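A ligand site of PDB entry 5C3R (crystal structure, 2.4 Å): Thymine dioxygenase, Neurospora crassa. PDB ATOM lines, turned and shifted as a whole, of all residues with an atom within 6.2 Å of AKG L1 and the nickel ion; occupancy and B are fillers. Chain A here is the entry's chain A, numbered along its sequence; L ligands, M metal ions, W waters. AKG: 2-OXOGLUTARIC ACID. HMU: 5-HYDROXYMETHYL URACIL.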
ATOM      1  N   LYS A 120       0.458  15.109  -9.654  1.00  0.00           N
ATOM      2  CA  LYS A 120       0.072  13.707  -9.744  1.00  0.00           C
ATOM      3  C   LYS A 120      -0.926  13.480 -10.862  1.00  0.00           C
ATOM      4  O   LYS A 120      -1.513  14.421 -11.393  1.00  0.00           O
ATOM      5  CB  LYS A 120      -0.519  13.229  -8.409  1.00  0.00           C
ATOM      6  CG  LYS A 120      -1.896  13.806  -8.069  1.00  0.00           C
ATOM      7  CD  LYS A 120      -2.302  13.488  -6.630  1.00  0.00           C
ATOM      8  CE  LYS A 120      -3.742  13.892  -6.348  1.00  0.00           C
ATOM      9  NZ  LYS A 120      -4.711  12.828  -6.756  1.00  0.00           N
ATOM     10  N   ARG A 192      -7.053   2.601  -7.149  1.00  0.00           N
ATOM     11  CA  ARG A 192      -6.493   3.838  -7.659  1.00  0.00           C
ATOM     12  C   ARG A 192      -5.020   3.659  -8.023  1.00  0.00           C
ATOM     13  O   ARG A 192      -4.174   3.506  -7.152  1.00  0.00           O
ATOM     14  CB  ARG A 192      -6.643   4.960  -6.627  1.00  0.00           C
ATOM     15  CG  ARG A 192      -6.031   6.296  -7.063  1.00  0.00           C
ATOM     16  CD  ARG A 192      -6.057   7.347  -5.975  1.00  0.00           C
ATOM     17  NE  ARG A 192      -7.215   8.241  -6.065  1.00  0.00           N
ATOM     18  CZ  ARG A 192      -7.424   9.307  -5.284  1.00  0.00           C
ATOM     19  NH1 ARG A 192      -6.563   9.617  -4.306  1.00  0.00           N
ATOM     20  NH2 ARG A 192      -8.499  10.053  -5.461  1.00  0.00           N
ATOM     21  N   LEU A 194      -1.655   5.359  -9.275  1.00  0.00           N
ATOM     22  CA  LEU A 194      -1.111   6.699  -9.110  1.00  0.00           C
ATOM     23  C   LEU A 194       0.257   6.819  -9.758  1.00  0.00           C
ATOM     24  O   LEU A 194       1.084   5.919  -9.659  1.00  0.00           O
ATOM     25  CB  LEU A 194      -0.990   7.060  -7.623  1.00  0.00           C
ATOM     26  CG  LEU A 194      -2.269   7.523  -6.927  1.00  0.00           C
ATOM     27  CD1 LEU A 194      -2.217   7.212  -5.432  1.00  0.00           C
ATOM     28  CD2 LEU A 194      -2.478   9.006  -7.161  1.00  0.00           C
ATOM     29  N   TYR A 196       3.160   9.916  -9.898  1.00  0.00           N
ATOM     30  CA  TYR A 196       3.660  11.235  -9.540  1.00  0.00           C
ATOM     31  C   TYR A 196       4.877  11.481 -10.425  1.00  0.00           C
ATOM     32  O   TYR A 196       5.944  10.913 -10.168  1.00  0.00           O
ATOM     33  CB  TYR A 196       4.060  11.282  -8.057  1.00  0.00           C
ATOM     34  CG  TYR A 196       2.955  10.925  -7.074  1.00  0.00           C
ATOM     35  CD1 TYR A 196       2.144  11.913  -6.526  1.00  0.00           C
ATOM     36  CD2 TYR A 196       2.743   9.618  -6.666  1.00  0.00           C
ATOM     37  CE1 TYR A 196       1.138  11.601  -5.624  1.00  0.00           C
ATOM     38  CE2 TYR A 196       1.728   9.292  -5.769  1.00  0.00           C
ATOM     39  CZ  TYR A 196       0.937  10.292  -5.250  1.00  0.00           C
ATOM     40  OH  TYR A 196      -0.049   9.989  -4.348  1.00  0.00           O
ATOM     41  N   ALA A 213       0.819  14.891  -2.988  1.00  0.00           N
ATOM     42  CA  ALA A 213      -0.576  14.616  -2.631  1.00  0.00           C
ATOM     43  C   ALA A 213      -0.942  15.358  -1.349  1.00  0.00           C
ATOM     44  O   ALA A 213      -0.247  15.221  -0.346  1.00  0.00           O
ATOM     45  CB  ALA A 213      -0.822  13.134  -2.458  1.00  0.00           C
ATOM     46  N   HIS A 216      -4.930  14.521   3.890  1.00  0.00           N
ATOM     47  CA  HIS A 216      -6.306  14.077   3.917  1.00  0.00           C
ATOM     48  C   HIS A 216      -6.423  12.853   4.802  1.00  0.00           C
ATOM     49  O   HIS A 216      -5.417  12.291   5.234  1.00  0.00           O
ATOM     50  CB  HIS A 216      -6.749  13.697   2.508  1.00  0.00           C
ATOM     51  CG  HIS A 216      -5.945  12.598   1.914  1.00  0.00           C
ATOM     52  ND1 HIS A 216      -4.666  12.788   1.418  1.00  0.00           N
ATOM     53  CD2 HIS A 216      -6.200  11.279   1.765  1.00  0.00           C
ATOM     54  CE1 HIS A 216      -4.193  11.643   0.963  1.00  0.00           C
ATOM     55  NE2 HIS A 216      -5.106  10.710   1.168  1.00  0.00           N
ATOM     56  N   THR A 217      -7.663  12.479   5.071  1.00  0.00           N
ATOM     57  CA  THR A 217      -7.985  11.160   5.583  1.00  0.00           C
ATOM     58  C   THR A 217      -8.693  10.420   4.468  1.00  0.00           C
ATOM     59  O   THR A 217      -9.408  11.037   3.668  1.00  0.00           O
ATOM     60  CB  THR A 217      -8.903  11.256   6.819  1.00  0.00           C
ATOM     61  OG1 THR A 217     -10.071  12.040   6.503  1.00  0.00           O
ATOM     62  CG2 THR A 217      -8.169  11.895   7.974  1.00  0.00           C
ATOM     63  N   ASP A 218      -8.495   9.106   4.389  1.00  0.00           N
ATOM     64  CA  ASP A 218      -9.275   8.256   3.478  1.00  0.00           C
ATOM     65  C   ASP A 218     -10.680   8.069   4.030  1.00  0.00           C
ATOM     66  O   ASP A 218     -10.914   8.239   5.233  1.00  0.00           O
ATOM     67  CB  ASP A 218      -8.611   6.893   3.285  1.00  0.00           C
ATOM     68  CG  ASP A 218      -7.236   6.986   2.622  1.00  0.00           C
ATOM     69  OD1 ASP A 218      -6.859   8.094   2.148  1.00  0.00           O
ATOM     70  OD2 ASP A 218      -6.543   5.955   2.584  1.00  0.00           O
ATOM     71  N   THR A 223      -7.499   1.060   3.492  1.00  0.00           N
ATOM     72  CA  THR A 223      -6.823   1.304   2.239  1.00  0.00           C
ATOM     73  C   THR A 223      -5.557   0.459   2.220  1.00  0.00           C
ATOM     74  O   THR A 223      -4.758   0.496   3.158  1.00  0.00           O
ATOM     75  CB  THR A 223      -6.456   2.790   2.085  1.00  0.00           C
ATOM     76  OG1 THR A 223      -7.654   3.561   2.042  1.00  0.00           O
ATOM     77  CG2 THR A 223      -5.665   3.041   0.803  1.00  0.00           C
ATOM     78  N   LEU A 225      -2.185   0.293   0.607  1.00  0.00           N
ATOM     79  CA  LEU A 225      -1.288   1.164  -0.128  1.00  0.00           C
ATOM     80  C   LEU A 225       0.026   0.465  -0.443  1.00  0.00           C
ATOM     81  O   LEU A 225       0.805   0.147   0.446  1.00  0.00           O
ATOM     82  CB  LEU A 225      -1.029   2.456   0.664  1.00  0.00           C
ATOM     83  CG  LEU A 225      -0.210   3.511  -0.067  1.00  0.00           C
ATOM     84  CD1 LEU A 225      -0.883   4.002  -1.335  1.00  0.00           C
ATOM     85  CD2 LEU A 225       0.053   4.678   0.861  1.00  0.00           C
ATOM     86  N   PHE A 226       0.234   0.236  -1.744  1.00  0.00           N
ATOM     87  CA  PHE A 226       1.447  -0.347  -2.282  1.00  0.00           C
ATOM     88  C   PHE A 226       2.292   0.816  -2.834  1.00  0.00           C
ATOM     89  O   PHE A 226       1.870   1.476  -3.787  1.00  0.00           O
ATOM     90  CB  PHE A 226       1.101  -1.312  -3.415  1.00  0.00           C
ATOM     91  CG  PHE A 226       0.128  -2.402  -3.032  1.00  0.00           C
ATOM     92  CD1 PHE A 226      -1.232  -2.174  -3.008  1.00  0.00           C
ATOM     93  CD2 PHE A 226       0.593  -3.673  -2.724  1.00  0.00           C
ATOM     94  CE1 PHE A 226      -2.119  -3.180  -2.676  1.00  0.00           C
ATOM     95  CE2 PHE A 226      -0.297  -4.694  -2.380  1.00  0.00           C
ATOM     96  CZ  PHE A 226      -1.657  -4.444  -2.361  1.00  0.00           C
ATOM     97  N   GLN A 227       3.446   1.069  -2.238  1.00  0.00           N
ATOM     98  CA  GLN A 227       4.323   2.158  -2.713  1.00  0.00           C
ATOM     99  C   GLN A 227       5.651   1.612  -3.222  1.00  0.00           C
ATOM    100  O   GLN A 227       6.126   0.574  -2.778  1.00  0.00           O
ATOM    101  CB  GLN A 227       4.561   3.200  -1.621  1.00  0.00           C
ATOM    102  CG  GLN A 227       5.251   2.684  -0.366  1.00  0.00           C
ATOM    103  CD  GLN A 227       5.609   3.792   0.609  1.00  0.00           C
ATOM    104  OE1 GLN A 227       5.715   4.963   0.232  1.00  0.00           O
ATOM    105  NE2 GLN A 227       5.798   3.415   1.871  1.00  0.00           N
ATOM    106  N   LEU A 233       5.662   9.580   1.310  1.00  0.00           N
ATOM    107  CA  LEU A 233       4.472   9.385   2.135  1.00  0.00           C
ATOM    108  C   LEU A 233       4.788   9.740   3.582  1.00  0.00           C
ATOM    109  O   LEU A 233       5.800   9.313   4.122  1.00  0.00           O
ATOM    110  CB  LEU A 233       3.965   7.949   2.039  1.00  0.00           C
ATOM    111  CG  LEU A 233       2.797   7.550   2.936  1.00  0.00           C
ATOM    112  CD1 LEU A 233       1.527   8.312   2.583  1.00  0.00           C
ATOM    113  CD2 LEU A 233       2.546   6.047   2.849  1.00  0.00           C
ATOM    114  N   ASN A 255      -4.065   1.348   6.150  1.00  0.00           N
ATOM    115  CA  ASN A 255      -4.607   2.333   7.057  1.00  0.00           C
ATOM    116  C   ASN A 255      -6.124   2.307   7.096  1.00  0.00           C
ATOM    117  O   ASN A 255      -6.778   2.020   6.100  1.00  0.00           O
ATOM    118  CB  ASN A 255      -4.111   3.736   6.696  1.00  0.00           C
ATOM    119  CG  ASN A 255      -4.605   4.195   5.349  1.00  0.00           C
ATOM    120  OD1 ASN A 255      -4.131   3.735   4.311  1.00  0.00           O
ATOM    121  ND2 ASN A 255      -5.544   5.132   5.353  1.00  0.00           N
ATOM    122  N   HIS A 273      -2.661  11.832   6.412  1.00  0.00           N
ATOM    123  CA  HIS A 273      -1.426  11.545   5.685  1.00  0.00           C
ATOM    124  C   HIS A 273      -1.351  12.358   4.391  1.00  0.00           C
ATOM    125  O   HIS A 273      -2.310  13.000   3.992  1.00  0.00           O
ATOM    126  CB  HIS A 273      -1.300  10.040   5.423  1.00  0.00           C
ATOM    127  CG  HIS A 273      -2.500   9.446   4.756  1.00  0.00           C
ATOM    128  ND1 HIS A 273      -3.707   9.307   5.402  1.00  0.00           N
ATOM    129  CD2 HIS A 273      -2.672   8.959   3.506  1.00  0.00           C
ATOM    130  CE1 HIS A 273      -4.579   8.776   4.566  1.00  0.00           C
ATOM    131  NE2 HIS A 273      -3.978   8.561   3.412  1.00  0.00           N
ATOM    132  N   ARG A 274      -0.188  12.335   3.755  1.00  0.00           N
ATOM    133  CA  ARG A 274       0.083  13.144   2.572  1.00  0.00           C
ATOM    134  C   ARG A 274       1.302  12.598   1.853  1.00  0.00           C
ATOM    135  O   ARG A 274       1.973  11.709   2.374  1.00  0.00           O
ATOM    136  CB  ARG A 274       0.326  14.597   2.973  1.00  0.00           C
ATOM    137  CG  ARG A 274       1.544  14.796   3.860  1.00  0.00           C
ATOM    138  CD  ARG A 274       1.781  16.255   4.185  1.00  0.00           C
ATOM    139  NE  ARG A 274       3.129  16.462   4.720  1.00  0.00           N
ATOM    140  CZ  ARG A 274       3.614  17.640   5.123  1.00  0.00           C
ATOM    141  NH1 ARG A 274       2.867  18.729   5.089  1.00  0.00           N
ATOM    142  NH2 ARG A 274       4.856  17.709   5.567  1.00  0.00           N
ATOM    143  N   VAL A 275       1.592  13.139   0.673  1.00  0.00           N
ATOM    144  CA  VAL A 275       2.821  12.828  -0.036  1.00  0.00           C
ATOM    145  C   VAL A 275       3.571  14.108  -0.395  1.00  0.00           C
ATOM    146  O   VAL A 275       3.066  14.942  -1.144  1.00  0.00           O
ATOM    147  CB  VAL A 275       2.556  12.006  -1.312  1.00  0.00           C
ATOM    148  CG1 VAL A 275       3.880  11.570  -1.930  1.00  0.00           C
ATOM    149  CG2 VAL A 275       1.708  10.784  -0.986  1.00  0.00           C
ATOM    150  N   ARG A 288       7.408   8.749  -9.149  1.00  0.00           N
ATOM    151  CA  ARG A 288       6.947   7.906  -8.055  1.00  0.00           C
ATOM    152  C   ARG A 288       5.637   7.227  -8.447  1.00  0.00           C
ATOM    153  O   ARG A 288       4.700   7.877  -8.913  1.00  0.00           O
ATOM    154  CB  ARG A 288       6.745   8.730  -6.776  1.00  0.00           C
ATOM    155  CG  ARG A 288       6.173   7.934  -5.616  1.00  0.00           C
ATOM    156  CD  ARG A 288       6.261   8.692  -4.301  1.00  0.00           C
ATOM    157  NE  ARG A 288       5.810   7.869  -3.179  1.00  0.00           N
ATOM    158  CZ  ARG A 288       4.541   7.705  -2.811  1.00  0.00           C
ATOM    159  NH1 ARG A 288       3.555   8.309  -3.464  1.00  0.00           N
ATOM    160  NH2 ARG A 288       4.245   6.913  -1.776  1.00  0.00           N
ATOM    161  N   SER A 290       2.597   4.615  -6.988  1.00  0.00           N
ATOM    162  CA  SER A 290       1.957   3.918  -5.898  1.00  0.00           C
ATOM    163  C   SER A 290       0.601   3.420  -6.381  1.00  0.00           C
ATOM    164  O   SER A 290       0.125   3.848  -7.433  1.00  0.00           O
ATOM    165  CB  SER A 290       1.801   4.815  -4.677  1.00  0.00           C
ATOM    166  OG  SER A 290       0.885   5.876  -4.921  1.00  0.00           O
ATOM    167  N   ILE A 291       0.004   2.514  -5.617  1.00  0.00           N
ATOM    168  CA  ILE A 291      -1.330   2.013  -5.883  1.00  0.00           C
ATOM    169  C   ILE A 291      -2.114   2.018  -4.583  1.00  0.00           C
ATOM    170  O   ILE A 291      -1.739   1.330  -3.612  1.00  0.00           O
ATOM    171  CB  ILE A 291      -1.295   0.582  -6.451  1.00  0.00           C
ATOM    172  CG1 ILE A 291      -0.530   0.557  -7.783  1.00  0.00           C
ATOM    173  CG2 ILE A 291      -2.718   0.058  -6.637  1.00  0.00           C
ATOM    174  CD1 ILE A 291      -0.435  -0.820  -8.414  1.00  0.00           C
ATOM    175  N   ALA A 292      -3.215   2.780  -4.565  1.00  0.00           N
ATOM    176  CA  ALA A 292      -4.102   2.844  -3.412  1.00  0.00           C
ATOM    177  C   ALA A 292      -5.369   2.076  -3.725  1.00  0.00           C
ATOM    178  O   ALA A 292      -6.157   2.490  -4.575  1.00  0.00           O
ATOM    179  CB  ALA A 292      -4.422   4.286  -3.065  1.00  0.00           C
ATOM    180  N   PHE A 294      -8.680   1.423  -2.298  1.00  0.00           N
ATOM    181  CA  PHE A 294      -9.611   1.873  -1.285  1.00  0.00           C
ATOM    182  C   PHE A 294     -10.660   0.795  -1.053  1.00  0.00           C
ATOM    183  O   PHE A 294     -11.400   0.442  -1.973  1.00  0.00           O
ATOM    184  CB  PHE A 294     -10.280   3.175  -1.717  1.00  0.00           C
ATOM    185  CG  PHE A 294      -9.311   4.290  -1.970  1.00  0.00           C
ATOM    186  CD1 PHE A 294      -8.482   4.745  -0.963  1.00  0.00           C
ATOM    187  CD2 PHE A 294      -9.225   4.893  -3.219  1.00  0.00           C
ATOM    188  CE1 PHE A 294      -7.581   5.771  -1.183  1.00  0.00           C
ATOM    189  CE2 PHE A 294      -8.334   5.919  -3.442  1.00  0.00           C
ATOM    190  CZ  PHE A 294      -7.506   6.365  -2.429  1.00  0.00           C
HETATM  191  C1  AKG L   1      -4.389   8.410  -1.545  1.00  0.00           C
HETATM  192  O1  AKG L   1      -5.410   8.499  -0.839  1.00  0.00           O
HETATM  193  O2  AKG L   1      -4.464   8.296  -2.785  1.00  0.00           O
HETATM  194  C2  AKG L   1      -3.069   8.446  -0.891  1.00  0.00           C
HETATM  195  O5  AKG L   1      -2.999   8.618   0.324  1.00  0.00           O
HETATM  196  C3  AKG L   1      -1.813   8.301  -1.743  1.00  0.00           C
HETATM  197  C4  AKG L   1      -0.580   7.949  -0.902  1.00  0.00           C
HETATM  198  C5  AKG L   1       0.602   7.555  -1.764  1.00  0.00           C
HETATM  199  O3  AKG L   1       1.569   7.020  -1.192  1.00  0.00           O
HETATM  200  O4  AKG L   1       0.608   7.771  -3.004  1.00  0.00           O
HETATM  201  N1  HMU L   2     -10.980   8.349  -3.202  1.00  0.00           N
HETATM  202  C2  HMU L   2     -11.707   7.218  -2.629  1.00  0.00           C
HETATM  203  O2  HMU L   2     -12.478   6.576  -3.302  1.00  0.00           O
HETATM  204  N3  HMU L   2     -11.488   6.866  -1.211  1.00  0.00           N
HETATM  205  C4  HMU L   2     -10.572   7.628  -0.430  1.00  0.00           C
HETATM  206  O3  HMU L   2      -7.708   9.809  -1.003  1.00  0.00           O
HETATM  207  O4  HMU L   2     -10.404   7.324   0.722  1.00  0.00           O
HETATM  208  C5  HMU L   2      -9.847   8.754  -1.027  1.00  0.00           C
HETATM  209  CM5 HMU L   2      -8.869   9.585  -0.224  1.00  0.00           C
HETATM  210  C6  HMU L   2     -10.071   9.096  -2.425  1.00  0.00           C
HETATM  211 NI    NI M   1      -4.847   8.429   1.276  1.00  0.00          NI
HETATM  212  O   HOH W   1      -4.387   6.220   1.212  1.00  0.00           O
HETATM  213  O   HOH W   2      -2.946  10.478  -4.068  1.00  0.00           O
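The side-chain carboxylate (OD2) of Asp 218 lies within hydrogen-bond range of the side-chain amide nitrogen (ND2) of Asn 255, at 3.1 Å.
The side-chain hydroxyl (OG1) of Thr 223 sits at hydrogen-bond distance from the side-chain carboxylate (OD2) of Asp 218 (2.7 Å).
The backbone NH (N) of Tyr 196 lies within hydrogen-bond range of the backbone carbonyl oxygen (O) of Arg 288.
N of Leu 194 is in hydrogen-bond range of O of Ser 290 (3.0 Å).
NH2 of Arg 288 lies within hydrogen-bond range of OE1 of Gln 227 (3.2 Å).
The backbone carbonyl oxygen (O) of Ala 292 sits at hydrogen-bond distance from the backbone NH (N) of Arg 192.
O of Val 275 lies within hydrogen-bond range of N of Ala 213, at 2.9 Å.
Leu 194 touches AKG L1.
Leu 225 touches AKG L1.
CD1 of Leu 233 touches O3 of AKG L1 (3.99 Å).
Val 275 touches AKG L1 (CG2 to C5, 3.5 Å).
CZ of Phe 294 touches O1 of AKG L1, at 3.4 Å.
Of the 22 residues printed, 12 come within 4 Å of AKG L1.
An oxygen (O3) of HMU L2 lies close to an oxygen (O1) of AKG L1, at 2.7 Å.
An oxygen (O4) of AKG L1 lies within hydrogen-bond range of the side-chain hydroxyl (OH) of Tyr 196, at 2.7 Å.
An oxygen (O4) of AKG L1 lies within hydrogen-bond range of the side-chain hydroxyl (OG) of Ser 290, 2.7 Å away.
The guanidinium group (NH2) of Arg 288 is in salt-bridge range of an oxygen (O3) of AKG L1, 2.7 Å away.
The guanidinium group of Arg 192 lies within salt-bridge range of an oxygen (O2) of AKG L1 (2.9 Å).
Of the 22 residues printed, 3 come within 4 Å of the nickel ion.
O5 of AKG L1 is bound to the nickel ion.
O1 of AKG L1 is bound to the nickel ion.
The nickel ion is bound by OD1 of Asp 218 (2.2 Å).
The nickel ion is bound by water W1, at 2.3 Å.
A ring nitrogen (NE2) of His 216 binds the nickel ion, 2.3 Å away.
The nickel ion is bound by NE2 of His 273 (2.3 Å).
The nickel ion has six donor atoms within binding distance.
Water W2 lies within hydrogen-bond range of the side-chain hydroxyl of Tyr 196 (3.0 Å) and an oxygen (O2) of AKG L1 (3.0 Å).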
